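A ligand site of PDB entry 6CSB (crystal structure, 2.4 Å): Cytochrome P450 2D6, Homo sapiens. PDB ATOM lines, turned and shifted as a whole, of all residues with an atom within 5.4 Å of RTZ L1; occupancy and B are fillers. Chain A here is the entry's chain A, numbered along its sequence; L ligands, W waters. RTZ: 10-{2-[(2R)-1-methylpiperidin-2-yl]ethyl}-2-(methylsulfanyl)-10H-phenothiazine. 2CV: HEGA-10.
A sulfur (SAX) of RTZ L1 sits close to the side-chain hydroxyl (OG) of Ser 282 (3.4 Å).
O of Ala 283 lies close to O44 of 2CV L2, at 2.8 Å.
A nitrogen (NAV) of RTZ L1 is in salt-bridge range of the side-chain carboxylate (OD2) of Asp 279, 2.7 Å away.
The side-chain amide nitrogen (NE2) of Gln 222 sits close to a sulfur (SAX) of RTZ L1.
SAY of RTZ L1 lies close to O51 of 2CV L2 (3.2 Å).
The side-chain carboxylate of Asp 279 lies within hydrogen-bond range of the backbone NH of Phe 98.
OG of Ser 282 lies within hydrogen-bond range of O of Ala 278 (3.0 Å).
The side-chain amide nitrogen of Gln 222 is in hydrogen-bond range of the backbone carbonyl oxygen of Gly 190 (2.9 Å).
OE1 of Glu 194 is in hydrogen-bond range of NE2 of Gln 222, 3.5 Å away.
The backbone carbonyl oxygen (O) of Gly 190 sits close to a sulfur (SAX) of RTZ L1.
Merely in contact with RTZ L1: Glu 194, Ala 187, Phe 98, Leu 99, Phe 90, Leu 191 and Leu 88.
Of the 20 residues printed, 11 come within 4 Å of RTZ L1.
Water W1 lies within hydrogen-bond range of the side-chain carboxylate of Asp 279 (2.7 Å) and the backbone NH of Leu 99 (3.1 Å).
Water W2 bridges the side-chain amide oxygen of Gln 222 (3.1 Å) and the side-chain carboxylate of Glu 194 (3.3 Å).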
ATOM      1  N   THR A  85     -28.322  -9.340 -29.022  1.00  0.00           N
ATOM      2  CA  THR A  85     -26.987  -9.652 -28.511  1.00  0.00           C
ATOM      3  C   THR A  85     -26.041 -10.103 -29.623  1.00  0.00           C
ATOM      4  O   THR A  85     -24.821 -10.110 -29.413  1.00  0.00           O
ATOM      5  CB  THR A  85     -27.013 -10.738 -27.452  1.00  0.00           C
ATOM      6  OG1 THR A  85     -27.454 -11.967 -28.053  1.00  0.00           O
ATOM      7  CG2 THR A  85     -27.906 -10.357 -26.278  1.00  0.00           C
ATOM      8  N   LEU A  88     -23.236  -7.889 -30.068  1.00  0.00           N
ATOM      9  CA  LEU A  88     -22.166  -7.754 -29.090  1.00  0.00           C
ATOM     10  C   LEU A  88     -21.213  -8.953 -29.044  1.00  0.00           C
ATOM     11  O   LEU A  88     -20.561  -9.173 -28.014  1.00  0.00           O
ATOM     12  CB  LEU A  88     -22.754  -7.511 -27.693  1.00  0.00           C
ATOM     13  CG  LEU A  88     -23.811  -6.427 -27.616  1.00  0.00           C
ATOM     14  CD1 LEU A  88     -24.369  -6.347 -26.198  1.00  0.00           C
ATOM     15  CD2 LEU A  88     -23.226  -5.117 -28.040  1.00  0.00           C
ATOM     16  N   PHE A  90     -21.956 -12.251 -29.471  1.00  0.00           N
ATOM     17  CA  PHE A  90     -22.552 -13.473 -28.933  1.00  0.00           C
ATOM     18  C   PHE A  90     -22.501 -14.593 -29.955  1.00  0.00           C
ATOM     19  O   PHE A  90     -22.866 -14.411 -31.126  1.00  0.00           O
ATOM     20  CB  PHE A  90     -23.995 -13.220 -28.529  1.00  0.00           C
ATOM     21  CG  PHE A  90     -24.166 -12.870 -27.094  1.00  0.00           C
ATOM     22  CD1 PHE A  90     -24.929 -13.686 -26.266  1.00  0.00           C
ATOM     23  CD2 PHE A  90     -23.602 -11.723 -26.561  1.00  0.00           C
ATOM     24  CE1 PHE A  90     -25.098 -13.378 -24.929  1.00  0.00           C
ATOM     25  CE2 PHE A  90     -23.769 -11.382 -25.226  1.00  0.00           C
ATOM     26  CZ  PHE A  90     -24.527 -12.211 -24.403  1.00  0.00           C
ATOM     27  N   PHE A  98     -24.722 -14.295 -17.936  1.00  0.00           N
ATOM     28  CA  PHE A  98     -26.017 -13.741 -17.539  1.00  0.00           C
ATOM     29  C   PHE A  98     -27.143 -14.168 -18.490  1.00  0.00           C
ATOM     30  O   PHE A  98     -28.173 -14.701 -18.067  1.00  0.00           O
ATOM     31  CB  PHE A  98     -25.902 -12.212 -17.485  1.00  0.00           C
ATOM     32  CG  PHE A  98     -27.011 -11.540 -16.707  1.00  0.00           C
ATOM     33  CD1 PHE A  98     -26.911 -11.389 -15.337  1.00  0.00           C
ATOM     34  CD2 PHE A  98     -28.135 -11.038 -17.359  1.00  0.00           C
ATOM     35  CE1 PHE A  98     -27.931 -10.764 -14.606  1.00  0.00           C
ATOM     36  CE2 PHE A  98     -29.156 -10.398 -16.645  1.00  0.00           C
ATOM     37  CZ  PHE A  98     -29.050 -10.263 -15.271  1.00  0.00           C
ATOM     38  N   LEU A  99     -27.007 -13.883 -19.787  1.00  0.00           N
ATOM     39  CA  LEU A  99     -28.040 -14.219 -20.746  1.00  0.00           C
ATOM     40  C   LEU A  99     -27.762 -15.527 -21.486  1.00  0.00           C
ATOM     41  O   LEU A  99     -28.502 -15.853 -22.413  1.00  0.00           O
ATOM     42  CB  LEU A  99     -28.210 -13.089 -21.762  1.00  0.00           C
ATOM     43  CG  LEU A  99     -28.714 -11.752 -21.222  1.00  0.00           C
ATOM     44  CD1 LEU A  99     -28.801 -10.714 -22.340  1.00  0.00           C
ATOM     45  CD2 LEU A  99     -30.077 -11.939 -20.547  1.00  0.00           C
ATOM     46  N   LEU A 186     -21.015   5.561 -19.366  1.00  0.00           N
ATOM     47  CA  LEU A 186     -21.443   4.643 -20.418  1.00  0.00           C
ATOM     48  C   LEU A 186     -22.274   3.506 -19.835  1.00  0.00           C
ATOM     49  O   LEU A 186     -23.276   3.098 -20.427  1.00  0.00           O
ATOM     50  CB  LEU A 186     -20.218   4.100 -21.158  1.00  0.00           C
ATOM     51  CG  LEU A 186     -19.314   5.145 -21.808  1.00  0.00           C
ATOM     52  CD1 LEU A 186     -17.945   4.548 -22.086  1.00  0.00           C
ATOM     53  CD2 LEU A 186     -19.957   5.670 -23.086  1.00  0.00           C
ATOM     54  N   ALA A 187     -21.873   3.004 -18.669  1.00  0.00           N
ATOM     55  CA  ALA A 187     -22.631   1.943 -18.009  1.00  0.00           C
ATOM     56  C   ALA A 187     -24.042   2.403 -17.662  1.00  0.00           C
ATOM     57  O   ALA A 187     -25.005   1.651 -17.836  1.00  0.00           O
ATOM     58  CB  ALA A 187     -21.904   1.491 -16.743  1.00  0.00           C
ATOM     59  N   GLN A 188     -24.182   3.625 -17.155  1.00  0.00           N
ATOM     60  CA  GLN A 188     -25.512   4.141 -16.836  1.00  0.00           C
ATOM     61  C   GLN A 188     -26.375   4.285 -18.089  1.00  0.00           C
ATOM     62  O   GLN A 188     -27.535   3.873 -18.102  1.00  0.00           O
ATOM     63  CB  GLN A 188     -25.371   5.481 -16.091  1.00  0.00           C
ATOM     64  CG  GLN A 188     -26.612   6.343 -16.039  1.00  0.00           C
ATOM     65  CD  GLN A 188     -26.495   7.572 -16.931  1.00  0.00           C
ATOM     66  OE1 GLN A 188     -25.404   7.961 -17.335  1.00  0.00           O
ATOM     67  NE2 GLN A 188     -27.629   8.229 -17.181  1.00  0.00           N
ATOM     68  N   GLY A 190     -26.025   2.632 -20.912  1.00  0.00           N
ATOM     69  CA  GLY A 190     -26.268   1.310 -21.463  1.00  0.00           C
ATOM     70  C   GLY A 190     -27.249   0.470 -20.670  1.00  0.00           C
ATOM     71  O   GLY A 190     -27.759  -0.524 -21.195  1.00  0.00           O
ATOM     72  N   LEU A 191     -27.500   0.840 -19.401  1.00  0.00           N
ATOM     73  CA  LEU A 191     -28.630   0.265 -18.685  1.00  0.00           C
ATOM     74  C   LEU A 191     -29.944   0.797 -19.235  1.00  0.00           C
ATOM     75  O   LEU A 191     -30.925   0.048 -19.371  1.00  0.00           O
ATOM     76  CB  LEU A 191     -28.516   0.557 -17.193  1.00  0.00           C
ATOM     77  CG  LEU A 191     -29.722   0.215 -16.304  1.00  0.00           C
ATOM     78  CD1 LEU A 191     -30.124  -1.250 -16.456  1.00  0.00           C
ATOM     79  CD2 LEU A 191     -29.441   0.556 -14.852  1.00  0.00           C
ATOM     80  N   GLU A 194     -31.251  -1.026 -22.160  1.00  0.00           N
ATOM     81  CA  GLU A 194     -31.880  -2.316 -21.868  1.00  0.00           C
ATOM     82  C   GLU A 194     -33.396  -2.197 -21.806  1.00  0.00           C
ATOM     83  O   GLU A 194     -34.108  -3.168 -22.077  1.00  0.00           O
ATOM     84  CB  GLU A 194     -31.353  -2.881 -20.549  1.00  0.00           C
ATOM     85  CG  GLU A 194     -30.138  -3.785 -20.681  1.00  0.00           C
ATOM     86  CD  GLU A 194     -30.433  -5.051 -21.428  1.00  0.00           C
ATOM     87  OE1 GLU A 194     -29.657  -5.406 -22.339  1.00  0.00           O
ATOM     88  OE2 GLU A 194     -31.456  -5.695 -21.104  1.00  0.00           O
ATOM     89  N   GLN A 222     -23.824   0.552 -25.007  1.00  0.00           N
ATOM     90  CA  GLN A 222     -23.231  -0.701 -24.579  1.00  0.00           C
ATOM     91  C   GLN A 222     -21.961  -0.992 -25.356  1.00  0.00           C
ATOM     92  O   GLN A 222     -20.925  -1.338 -24.776  1.00  0.00           O
ATOM     93  CB  GLN A 222     -24.250  -1.835 -24.720  1.00  0.00           C
ATOM     94  CG  GLN A 222     -25.495  -1.650 -23.851  1.00  0.00           C
ATOM     95  CD  GLN A 222     -26.214  -2.951 -23.571  1.00  0.00           C
ATOM     96  OE1 GLN A 222     -25.828  -4.013 -24.065  1.00  0.00           O
ATOM     97  NE2 GLN A 222     -27.278  -2.876 -22.772  1.00  0.00           N
ATOM     98  N   PHE A 225     -19.362   1.134 -23.977  1.00  0.00           N
ATOM     99  CA  PHE A 225     -18.963   0.497 -22.731  1.00  0.00           C
ATOM    100  C   PHE A 225     -17.997  -0.646 -23.005  1.00  0.00           C
ATOM    101  O   PHE A 225     -16.895  -0.671 -22.457  1.00  0.00           O
ATOM    102  CB  PHE A 225     -20.198   0.001 -21.986  1.00  0.00           C
ATOM    103  CG  PHE A 225     -19.891  -0.648 -20.664  1.00  0.00           C
ATOM    104  CD1 PHE A 225     -19.444   0.112 -19.599  1.00  0.00           C
ATOM    105  CD2 PHE A 225     -20.043  -2.004 -20.498  1.00  0.00           C
ATOM    106  CE1 PHE A 225     -19.163  -0.475 -18.382  1.00  0.00           C
ATOM    107  CE2 PHE A 225     -19.752  -2.594 -19.284  1.00  0.00           C
ATOM    108  CZ  PHE A 225     -19.317  -1.828 -18.224  1.00  0.00           C
ATOM    109  N   LEU A 226     -18.393  -1.581 -23.898  1.00  0.00           N
ATOM    110  CA  LEU A 226     -17.522  -2.701 -24.237  1.00  0.00           C
ATOM    111  C   LEU A 226     -16.176  -2.234 -24.784  1.00  0.00           C
ATOM    112  O   LEU A 226     -15.135  -2.802 -24.452  1.00  0.00           O
ATOM    113  CB  LEU A 226     -18.221  -3.631 -25.231  1.00  0.00           C
ATOM    114  CG  LEU A 226     -19.249  -4.560 -24.579  1.00  0.00           C
ATOM    115  CD1 LEU A 226     -20.244  -5.107 -25.599  1.00  0.00           C
ATOM    116  CD2 LEU A 226     -18.540  -5.687 -23.814  1.00  0.00           C
ATOM    117  N   ILE A 275     -17.424 -10.497 -22.646  1.00  0.00           N
ATOM    118  CA  ILE A 275     -18.828 -10.562 -22.269  1.00  0.00           C
ATOM    119  C   ILE A 275     -18.955 -10.978 -20.808  1.00  0.00           C
ATOM    120  O   ILE A 275     -19.778 -10.416 -20.063  1.00  0.00           O
ATOM    121  CB  ILE A 275     -19.605 -11.484 -23.208  1.00  0.00           C
ATOM    122  CG1 ILE A 275     -19.631 -10.858 -24.611  1.00  0.00           C
ATOM    123  CG2 ILE A 275     -21.029 -11.695 -22.695  1.00  0.00           C
ATOM    124  CD1 ILE A 275     -20.034 -11.826 -25.694  1.00  0.00           C
ATOM    125  N   ALA A 278     -18.088  -7.908 -18.740  1.00  0.00           N
ATOM    126  CA  ALA A 278     -19.169  -6.944 -18.831  1.00  0.00           C
ATOM    127  C   ALA A 278     -20.441  -7.409 -18.099  1.00  0.00           C
ATOM    128  O   ALA A 278     -21.197  -6.564 -17.579  1.00  0.00           O
ATOM    129  CB  ALA A 278     -19.472  -6.644 -20.296  1.00  0.00           C
ATOM    130  N   ASP A 279     -20.720  -8.714 -18.077  1.00  0.00           N
ATOM    131  CA  ASP A 279     -21.858  -9.207 -17.292  1.00  0.00           C
ATOM    132  C   ASP A 279     -21.658  -8.956 -15.802  1.00  0.00           C
ATOM    133  O   ASP A 279     -22.599  -8.604 -15.074  1.00  0.00           O
ATOM    134  CB  ASP A 279     -22.038 -10.707 -17.546  1.00  0.00           C
ATOM    135  CG  ASP A 279     -22.782 -11.006 -18.841  1.00  0.00           C
ATOM    136  OD1 ASP A 279     -22.955 -12.198 -19.147  1.00  0.00           O
ATOM    137  OD2 ASP A 279     -23.177 -10.063 -19.549  1.00  0.00           O
ATOM    138  N   SER A 282     -22.301  -5.332 -15.170  1.00  0.00           N
ATOM    139  CA  SER A 282     -23.694  -5.010 -15.426  1.00  0.00           C
ATOM    140  C   SER A 282     -24.600  -5.520 -14.322  1.00  0.00           C
ATOM    141  O   SER A 282     -25.524  -4.839 -13.880  1.00  0.00           O
ATOM    142  CB  SER A 282     -24.123  -5.624 -16.755  1.00  0.00           C
ATOM    143  OG  SER A 282     -23.620  -4.881 -17.814  1.00  0.00           O
ATOM    144  N   ALA A 283     -24.376  -6.760 -13.910  1.00  0.00           N
ATOM    145  CA  ALA A 283     -25.214  -7.378 -12.898  1.00  0.00           C
ATOM    146  C   ALA A 283     -24.847  -6.937 -11.483  1.00  0.00           C
ATOM    147  O   ALA A 283     -25.705  -6.977 -10.590  1.00  0.00           O
ATOM    148  CB  ALA A 283     -25.112  -8.913 -13.011  1.00  0.00           C
ATOM    149  N   VAL A 352     -35.307 -11.643 -13.280  1.00  0.00           N
ATOM    150  CA  VAL A 352     -34.746 -11.758 -14.622  1.00  0.00           C
ATOM    151  C   VAL A 352     -35.466 -12.919 -15.301  1.00  0.00           C
ATOM    152  O   VAL A 352     -35.630 -13.988 -14.705  1.00  0.00           O
ATOM    153  CB  VAL A 352     -33.217 -11.988 -14.591  1.00  0.00           C
ATOM    154  CG1 VAL A 352     -32.627 -12.220 -15.996  1.00  0.00           C
ATOM    155  CG2 VAL A 352     -32.529 -10.851 -13.879  1.00  0.00           C
HETATM  156  CAA RTZ L   1     -25.335  -9.813 -21.759  1.00  0.00           C
HETATM  157  CAB RTZ L   1     -24.262  -1.313 -19.110  1.00  0.00           C
HETATM  158  CAC RTZ L   1     -31.189  -8.162 -18.737  1.00  0.00           C
HETATM  159  CAD RTZ L   1     -31.580  -7.791 -17.474  1.00  0.00           C
HETATM  160  CAE RTZ L   1     -23.075  -6.206 -22.185  1.00  0.00           C
HETATM  161  CAF RTZ L   1     -22.594  -7.476 -22.860  1.00  0.00           C
HETATM  162  CAG RTZ L   1     -23.733  -6.514 -20.842  1.00  0.00           C
HETATM  163  CAH RTZ L   1     -29.915  -7.865 -19.195  1.00  0.00           C
HETATM  164  CAI RTZ L   1     -30.709  -7.121 -16.643  1.00  0.00           C
HETATM  165  CAJ RTZ L   1     -26.338  -2.942 -17.779  1.00  0.00           C
HETATM  166  CAK RTZ L   1     -27.068  -3.696 -16.877  1.00  0.00           C
HETATM  167  CAL RTZ L   1     -25.604  -7.744 -19.686  1.00  0.00           C
HETATM  168  CAM RTZ L   1     -23.713  -8.500 -22.964  1.00  0.00           C
HETATM  169  CAN RTZ L   1     -27.099  -7.556 -19.911  1.00  0.00           C
HETATM  170  CAO RTZ L   1     -26.546  -4.694 -19.408  1.00  0.00           C
HETATM  171  CAP RTZ L   1     -24.872  -7.517 -21.019  1.00  0.00           C
HETATM  172  CAQ RTZ L   1     -26.061  -3.449 -19.040  1.00  0.00           C
HETATM  173  CAR RTZ L   1     -29.028  -7.166 -18.383  1.00  0.00           C
HETATM  174  CAS RTZ L   1     -27.259  -5.476 -18.519  1.00  0.00           C
HETATM  175  CAT RTZ L   1     -29.427  -6.806 -17.099  1.00  0.00           C
HETATM  176  CAU RTZ L   1     -27.502  -4.967 -17.234  1.00  0.00           C
HETATM  177  NAV RTZ L   1     -24.334  -8.743 -21.654  1.00  0.00           N
HETATM  178  NAW RTZ L   1     -27.772  -6.743 -18.875  1.00  0.00           N
HETATM  179  SAX RTZ L   1     -24.891  -2.660 -20.092  1.00  0.00           S
HETATM  180  SAY RTZ L   1     -28.334  -5.944 -16.026  1.00  0.00           S
HETATM  181  N33 2CV L   2     -34.467  -6.135 -13.705  1.00  0.00           N
HETATM  182  C36 2CV L   2     -33.301  -6.413 -14.525  1.00  0.00           C
HETATM  183  C37 2CV L   2     -32.430  -7.406 -13.754  1.00  0.00           C
HETATM  184  C40 2CV L   2     -31.417  -6.730 -12.831  1.00  0.00           C
HETATM  185  C41 2CV L   2     -30.002  -7.317 -12.882  1.00  0.00           C
HETATM  186  C42 2CV L   2     -29.641  -8.178 -11.668  1.00  0.00           C
HETATM  187  C43 2CV L   2     -28.258  -8.773 -11.853  1.00  0.00           C
HETATM  188  O44 2CV L   2     -27.606  -9.071 -10.620  1.00  0.00           O
HETATM  189  O51 2CV L   2     -29.039  -6.257 -12.953  1.00  0.00           O
HETATM  190  O53 2CV L   2     -30.551  -9.264 -11.523  1.00  0.00           O
HETATM  191  CAA RTZ L   3     -40.765  -6.793 -22.622  1.00  0.00           C
HETATM  192  CAB RTZ L   3     -34.351  -9.738 -19.313  1.00  0.00           C
HETATM  193  CAC RTZ L   3     -39.362  -3.999 -20.239  1.00  0.00           C
HETATM  194  CAD RTZ L   3     -40.122  -3.650 -19.131  1.00  0.00           C
HETATM  195  CAE RTZ L   3     -41.224 -10.858 -23.828  1.00  0.00           C
HETATM  196  CAF RTZ L   3     -41.696  -9.715 -24.717  1.00  0.00           C
HETATM  197  CAG RTZ L   3     -41.285 -10.479 -22.350  1.00  0.00           C
HETATM  198  CAH RTZ L   3     -38.895  -5.290 -20.391  1.00  0.00           C
HETATM  199  CAI RTZ L   3     -40.420  -4.590 -18.161  1.00  0.00           C
HETATM  200  CAJ RTZ L   3     -36.567  -8.574 -15.983  1.00  0.00           C
HETATM  201  CAK RTZ L   3     -37.831  -8.008 -15.902  1.00  0.00           C
HETATM  202  CAL RTZ L   3     -40.331  -8.866 -20.638  1.00  0.00           C
HETATM  203  CAM RTZ L   3     -40.983  -8.418 -24.384  1.00  0.00           C
HETATM  204  CAN RTZ L   3     -38.876  -8.450 -20.552  1.00  0.00           C
HETATM  205  CAO RTZ L   3     -36.690  -8.538 -18.388  1.00  0.00           C
HETATM  206  CAP RTZ L   3     -40.510  -9.184 -22.120  1.00  0.00           C
HETATM  207  CAQ RTZ L   3     -36.002  -8.853 -17.223  1.00  0.00           C
HETATM  208  CAR RTZ L   3     -39.187  -6.246 -19.417  1.00  0.00           C
HETATM  209  CAS RTZ L   3     -37.949  -7.964 -18.307  1.00  0.00           C
HETATM  210  CAT RTZ L   3     -39.946  -5.896 -18.309  1.00  0.00           C
HETATM  211  CAU RTZ L   3     -38.529  -7.722 -17.063  1.00  0.00           C
HETATM  212  NAV RTZ L   3     -41.183  -8.154 -22.956  1.00  0.00           N
HETATM  213  NAW RTZ L   3     -38.624  -7.536 -19.443  1.00  0.00           N
HETATM  214  SAX RTZ L   3     -34.470  -9.672 -17.523  1.00  0.00           S
HETATM  215  SAY RTZ L   3     -40.165  -7.062 -17.006  1.00  0.00           S
HETATM  216  O   HOH W   1     -24.492 -12.938 -21.260  1.00  0.00           O
HETATM  217  O   HOH W   2     -27.033  -6.877 -23.632  1.00  0.00           O
